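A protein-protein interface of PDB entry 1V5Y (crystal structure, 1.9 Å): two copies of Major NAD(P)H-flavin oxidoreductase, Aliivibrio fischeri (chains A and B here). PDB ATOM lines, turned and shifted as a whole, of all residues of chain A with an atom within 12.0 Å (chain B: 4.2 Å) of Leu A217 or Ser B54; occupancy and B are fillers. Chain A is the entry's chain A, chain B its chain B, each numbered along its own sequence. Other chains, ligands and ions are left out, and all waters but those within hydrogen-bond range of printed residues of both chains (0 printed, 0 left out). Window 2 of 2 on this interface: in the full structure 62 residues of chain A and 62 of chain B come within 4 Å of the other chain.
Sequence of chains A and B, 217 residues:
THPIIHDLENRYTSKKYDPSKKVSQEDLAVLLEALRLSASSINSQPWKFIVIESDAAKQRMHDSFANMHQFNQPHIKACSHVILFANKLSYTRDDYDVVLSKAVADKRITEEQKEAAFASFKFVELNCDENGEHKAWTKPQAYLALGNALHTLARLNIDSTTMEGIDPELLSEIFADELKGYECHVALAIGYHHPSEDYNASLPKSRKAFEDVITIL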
ATOM      1  N   PHE A 210      20.069 -18.080  -1.986  1.00  0.00           N
ATOM      2  CA  PHE A 210      19.991 -16.777  -1.348  1.00  0.00           C
ATOM      3  C   PHE A 210      20.847 -16.700  -0.079  1.00  0.00           C
ATOM      4  O   PHE A 210      21.527 -15.700   0.158  1.00  0.00           O
ATOM      5  CB  PHE A 210      18.526 -16.496  -1.011  1.00  0.00           C
ATOM      6  CG  PHE A 210      18.286 -15.184  -0.304  1.00  0.00           C
ATOM      7  CD1 PHE A 210      17.731 -14.110  -0.988  1.00  0.00           C
ATOM      8  CD2 PHE A 210      18.579 -15.032   1.052  1.00  0.00           C
ATOM      9  CE1 PHE A 210      17.470 -12.914  -0.333  1.00  0.00           C
ATOM     10  CE2 PHE A 210      18.323 -13.844   1.710  1.00  0.00           C
ATOM     11  CZ  PHE A 210      17.768 -12.784   1.012  1.00  0.00           C
ATOM     12  N   GLU A 211      20.774 -17.744   0.744  1.00  0.00           N
ATOM     13  CA  GLU A 211      21.515 -17.821   2.006  1.00  0.00           C
ATOM     14  C   GLU A 211      23.035 -17.873   1.853  1.00  0.00           C
ATOM     15  O   GLU A 211      23.770 -17.472   2.744  1.00  0.00           O
ATOM     16  CB  GLU A 211      21.034 -19.029   2.816  1.00  0.00           C
ATOM     17  CG  GLU A 211      19.635 -18.861   3.414  1.00  0.00           C
ATOM     18  CD  GLU A 211      18.491 -19.125   2.438  1.00  0.00           C
ATOM     19  OE1 GLU A 211      18.714 -19.702   1.345  1.00  0.00           O
ATOM     20  OE2 GLU A 211      17.346 -18.762   2.783  1.00  0.00           O
ATOM     21  N   VAL A 213      24.778 -16.218  -0.513  1.00  0.00           N
ATOM     22  CA  VAL A 213      25.352 -14.953  -0.974  1.00  0.00           C
ATOM     23  C   VAL A 213      24.868 -13.744  -0.216  1.00  0.00           C
ATOM     24  O   VAL A 213      25.481 -12.685  -0.308  1.00  0.00           O
ATOM     25  CB  VAL A 213      25.096 -14.712  -2.502  1.00  0.00           C
ATOM     26  CG1 VAL A 213      25.844 -15.734  -3.316  1.00  0.00           C
ATOM     27  CG2 VAL A 213      23.590 -14.756  -2.821  1.00  0.00           C
ATOM     28  N   ILE A 214      23.772 -13.893   0.526  1.00  0.00           N
ATOM     29  CA  ILE A 214      23.213 -12.779   1.276  1.00  0.00           C
ATOM     30  C   ILE A 214      23.157 -13.052   2.782  1.00  0.00           C
ATOM     31  O   ILE A 214      22.689 -14.100   3.201  1.00  0.00           O
ATOM     32  CB  ILE A 214      21.797 -12.437   0.750  1.00  0.00           C
ATOM     33  CG1 ILE A 214      21.907 -11.975  -0.708  1.00  0.00           C
ATOM     34  CG2 ILE A 214      21.165 -11.335   1.613  1.00  0.00           C
ATOM     35  CD1 ILE A 214      20.625 -12.024  -1.473  1.00  0.00           C
ATOM     36  N   THR A 215      23.627 -12.093   3.575  1.00  0.00           N
ATOM     37  CA  THR A 215      23.631 -12.200   5.028  1.00  0.00           C
ATOM     38  C   THR A 215      22.948 -10.962   5.559  1.00  0.00           C
ATOM     39  O   THR A 215      23.320  -9.860   5.193  1.00  0.00           O
ATOM     40  CB  THR A 215      25.085 -12.222   5.601  1.00  0.00           C
ATOM     41  OG1 THR A 215      25.735 -13.443   5.230  1.00  0.00           O
ATOM     42  CG2 THR A 215      25.068 -12.127   7.120  1.00  0.00           C
ATOM     43  N   ILE A 216      21.941 -11.129   6.409  1.00  0.00           N
ATOM     44  CA  ILE A 216      21.258  -9.966   6.970  1.00  0.00           C
ATOM     45  C   ILE A 216      21.610  -9.857   8.456  1.00  0.00           C
ATOM     46  O   ILE A 216      21.456 -10.814   9.206  1.00  0.00           O
ATOM     47  CB  ILE A 216      19.734 -10.043   6.714  1.00  0.00           C
ATOM     48  CG1 ILE A 216      19.493 -10.101   5.197  1.00  0.00           C
ATOM     49  CG2 ILE A 216      19.031  -8.819   7.299  1.00  0.00           C
ATOM     50  CD1 ILE A 216      18.110 -10.476   4.772  1.00  0.00           C
ATOM     51  N   LEU A 217      22.111  -8.694   8.855  1.00  0.00           N
ATOM     52  CA  LEU A 217      22.543  -8.440  10.223  1.00  0.00           C
ATOM     53  C   LEU A 217      21.762  -7.338  10.944  1.00  0.00           C
ATOM     54  O   LEU A 217      21.802  -7.314  12.197  1.00  0.00           O
ATOM     55  CB  LEU A 217      24.040  -8.095  10.236  1.00  0.00           C
ATOM     56  CG  LEU A 217      25.042  -9.077   9.613  1.00  0.00           C
ATOM     57  CD1 LEU A 217      26.412  -8.411   9.648  1.00  0.00           C
ATOM     58  CD2 LEU A 217      25.063 -10.427  10.339  1.00  0.00           C
ATOM     59  OXT LEU A 217      21.147  -6.494  10.272  1.00  0.00           O
ATOM     60  N   ILE B  50      26.311  -8.187   2.300  1.00  0.00           N
ATOM     61  CA  ILE B  50      25.982  -8.110   3.709  1.00  0.00           C
ATOM     62  C   ILE B  50      25.075  -6.924   3.987  1.00  0.00           C
ATOM     63  O   ILE B  50      25.450  -5.771   3.765  1.00  0.00           O
ATOM     64  CB  ILE B  50      27.266  -8.027   4.544  1.00  0.00           C
ATOM     65  CG1 ILE B  50      28.116  -9.286   4.289  1.00  0.00           C
ATOM     66  CG2 ILE B  50      26.931  -7.865   6.031  1.00  0.00           C
ATOM     67  CD1 ILE B  50      29.573  -9.105   4.646  1.00  0.00           C
ATOM     68  N   VAL B  51      23.872  -7.216   4.476  1.00  0.00           N
ATOM     69  CA  VAL B  51      22.882  -6.186   4.759  1.00  0.00           C
ATOM     70  C   VAL B  51      22.896  -5.772   6.224  1.00  0.00           C
ATOM     71  O   VAL B  51      22.645  -6.575   7.100  1.00  0.00           O
ATOM     72  CB  VAL B  51      21.453  -6.660   4.375  1.00  0.00           C
ATOM     73  CG1 VAL B  51      20.483  -5.499   4.421  1.00  0.00           C
ATOM     74  CG2 VAL B  51      21.461  -7.331   3.016  1.00  0.00           C
ATOM     75  N   ILE B  52      23.181  -4.504   6.465  1.00  0.00           N
ATOM     76  CA  ILE B  52      23.227  -3.927   7.788  1.00  0.00           C
ATOM     77  C   ILE B  52      21.822  -3.368   8.009  1.00  0.00           C
ATOM     78  O   ILE B  52      21.471  -2.302   7.492  1.00  0.00           O
ATOM     79  CB  ILE B  52      24.262  -2.781   7.826  1.00  0.00           C
ATOM     80  CG1 ILE B  52      25.636  -3.252   7.308  1.00  0.00           C
ATOM     81  CG2 ILE B  52      24.336  -2.145   9.205  1.00  0.00           C
ATOM     82  CD1 ILE B  52      26.183  -4.471   7.969  1.00  0.00           C
ATOM     83  N   GLU B  53      21.023  -4.097   8.773  1.00  0.00           N
ATOM     84  CA  GLU B  53      19.638  -3.720   9.044  1.00  0.00           C
ATOM     85  C   GLU B  53      19.317  -3.359  10.504  1.00  0.00           C
ATOM     86  O   GLU B  53      18.705  -2.321  10.778  1.00  0.00           O
ATOM     87  CB  GLU B  53      18.725  -4.855   8.587  1.00  0.00           C
ATOM     88  CG  GLU B  53      17.267  -4.649   8.924  1.00  0.00           C
ATOM     89  CD  GLU B  53      16.385  -5.667   8.251  1.00  0.00           C
ATOM     90  OE1 GLU B  53      15.656  -5.302   7.315  1.00  0.00           O
ATOM     91  OE2 GLU B  53      16.426  -6.841   8.635  1.00  0.00           O
ATOM     92  N   SER B  54      19.749  -4.197  11.442  1.00  0.00           N
ATOM     93  CA  SER B  54      19.465  -3.962  12.860  1.00  0.00           C
ATOM     94  C   SER B  54      20.218  -2.773  13.438  1.00  0.00           C
ATOM     95  O   SER B  54      21.218  -2.317  12.877  1.00  0.00           O
ATOM     96  CB  SER B  54      19.788  -5.213  13.679  1.00  0.00           C
ATOM     97  OG  SER B  54      21.189  -5.378  13.838  1.00  0.00           O
ATOM     98  N   ASP B  55      19.723  -2.260  14.560  1.00  0.00           N
ATOM     99  CA  ASP B  55      20.375  -1.157  15.255  1.00  0.00           C
ATOM    100  C   ASP B  55      21.778  -1.553  15.719  1.00  0.00           C
ATOM    101  O   ASP B  55      22.699  -0.731  15.739  1.00  0.00           O
ATOM    102  CB  ASP B  55      19.559  -0.735  16.474  1.00  0.00           C
ATOM    103  CG  ASP B  55      18.453   0.240  16.129  1.00  0.00           C
ATOM    104  OD1 ASP B  55      18.159   0.434  14.926  1.00  0.00           O
ATOM    105  OD2 ASP B  55      17.881   0.831  17.070  1.00  0.00           O
ATOM    106  N   ALA B  56      21.924  -2.813  16.113  1.00  0.00           N
ATOM    107  CA  ALA B  56      23.200  -3.327  16.574  1.00  0.00           C
ATOM    108  C   ALA B  56      24.179  -3.362  15.401  1.00  0.00           C
ATOM    109  O   ALA B  56      25.324  -2.967  15.555  1.00  0.00           O
ATOM    110  CB  ALA B  56      23.021  -4.712  17.171  1.00  0.00           C
ATOM    111  N   ALA B  57      23.727  -3.848  14.244  1.00  0.00           N
ATOM    112  CA  ALA B  57      24.572  -3.899  13.053  1.00  0.00           C
ATOM    113  C   ALA B  57      24.934  -2.477  12.607  1.00  0.00           C
ATOM    114  O   ALA B  57      26.077  -2.224  12.251  1.00  0.00           O
ATOM    115  CB  ALA B  57      23.868  -4.670  11.928  1.00  0.00           C
ATOM    116  N   LYS B  58      23.980  -1.547  12.655  1.00  0.00           N
ATOM    117  CA  LYS B  58      24.234  -0.160  12.262  1.00  0.00           C
ATOM    118  C   LYS B  58      25.312   0.472  13.140  1.00  0.00           C
ATOM    119  O   LYS B  58      26.085   1.300  12.680  1.00  0.00           O
ATOM    120  CB  LYS B  58      22.967   0.696  12.368  1.00  0.00           C
ATOM    121  CG  LYS B  58      21.877   0.415  11.350  1.00  0.00           C
ATOM    122  CD  LYS B  58      22.244   0.955   9.992  1.00  0.00           C
ATOM    123  CE  LYS B  58      21.007   1.170   9.115  1.00  0.00           C
ATOM    124  NZ  LYS B  58      20.029   2.129   9.721  1.00  0.00           N
ATOM    125  N   PHE B 175      33.474  -6.857  11.166  1.00  0.00           N
ATOM    126  CA  PHE B 175      32.634  -7.907  10.591  1.00  0.00           C
ATOM    127  C   PHE B 175      33.524  -9.082  10.258  1.00  0.00           C
ATOM    128  O   PHE B 175      33.407  -9.713   9.208  1.00  0.00           O
ATOM    129  CB  PHE B 175      31.906  -7.396   9.338  1.00  0.00           C
ATOM    130  CG  PHE B 175      30.964  -6.268   9.624  1.00  0.00           C
ATOM    131  CD1 PHE B 175      31.342  -4.951   9.412  1.00  0.00           C
ATOM    132  CD2 PHE B 175      29.724  -6.524  10.174  1.00  0.00           C
ATOM    133  CE1 PHE B 175      30.512  -3.918   9.747  1.00  0.00           C
ATOM    134  CE2 PHE B 175      28.886  -5.492  10.513  1.00  0.00           C
ATOM    135  CZ  PHE B 175      29.276  -4.187  10.304  1.00  0.00           C
ATOM    136  N   GLU B 178      31.823 -12.463   9.146  1.00  0.00           N
ATOM    137  CA  GLU B 178      31.056 -12.266   7.921  1.00  0.00           C
ATOM    138  C   GLU B 178      31.942 -12.045   6.691  1.00  0.00           C
ATOM    139  O   GLU B 178      31.667 -12.577   5.621  1.00  0.00           O
ATOM    140  CB  GLU B 178      30.073 -11.103   8.101  1.00  0.00           C
ATOM    141  CG  GLU B 178      29.085 -11.293   9.270  1.00  0.00           C
ATOM    142  CD  GLU B 178      29.572 -10.712  10.618  1.00  0.00           C
ATOM    143  OE1 GLU B 178      30.786 -10.513  10.838  1.00  0.00           O
ATOM    144  OE2 GLU B 178      28.719 -10.453  11.489  1.00  0.00           O
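The backbone carbonyl oxygen of Thr A215 lies within hydrogen-bond range of the backbone NH of Val B51 (2.8 Å). N of Leu A217 lies within hydrogen-bond range of O of Val B51 (2.8 Å). N of Glu B53 sits at hydrogen-bond distance from OXT of Leu A217, at 2.8 Å. The side-chain hydroxyl (OG) of Ser B54 is in hydrogen-bond range of the chain-end carboxylate (O) of Leu A217.
OG of Ser B54 is in hydrogen-bond range of N of Ala B57 (3.0 Å).
O of Thr A215 touches CA of Ile B50, 3.5 Å away. CA of Ile A216 touches O of Val B51, 3.7 Å away. Glu B53 touches Ile A216. Ile B50 touches Leu A217. OXT of Leu A217 touches C of Ile B52, at 3.9 Å. O of Leu A217 touches CB of Ala B57 (3.4 Å). Phe B175 touches Leu A217. Glu B178 touches Leu A217 (OE2 to CD1, 3.6 Å).
Of the printed residues of chain B, Thr A215 touches Ile B50 and Val B51. Printed residues of chain B within 4 Å of Ile A216: Val B51 and Glu B53. Leu A217 touches eight residues of chain B. Of the printed residues of chain A, Val B51 touches Thr A215 (2.8 Å), Ile A216 (3.7 Å) and Leu A217 (2.8 Å). Ile B52 touches just one residue of chain A: Leu A217 (3.9 Å). Ser B54 touches one residue of chain A. No residue of chain A comes within 4 Å of Asp B55. No residue of chain A comes within 4 Å of Ala B56. No residue of chain A comes within 4 Å of Lys B58. Glu B178 touches one residue of chain A. The nearest printed residue of chain B that does not touch Leu A217 is Ala B56 (5.6 Å). The nearest residue of chain A that does not touch Ser B54 is Ile A216 (6.2 Å). The nearest printed residue of chain B that does not touch Thr A215 is Glu B178 (4.6 Å).
Hydrophobic or aromatic side chains of chain A that line the printed part of chain B: Ile A216 and Leu A217. Of the 11 printed residues of chain B, 8 touch a printed residue of chain A. Hydrophobic or aromatic side chains of chain B that line the printed part of chain A: Ile B50, Val B51, Ala B57 and Phe B175. Among the printed residues, no Asp or Glu carboxylate lies within 4 Å of a Lys or Arg side-chain nitrogen of the other chain.
No position is printed for both chains.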
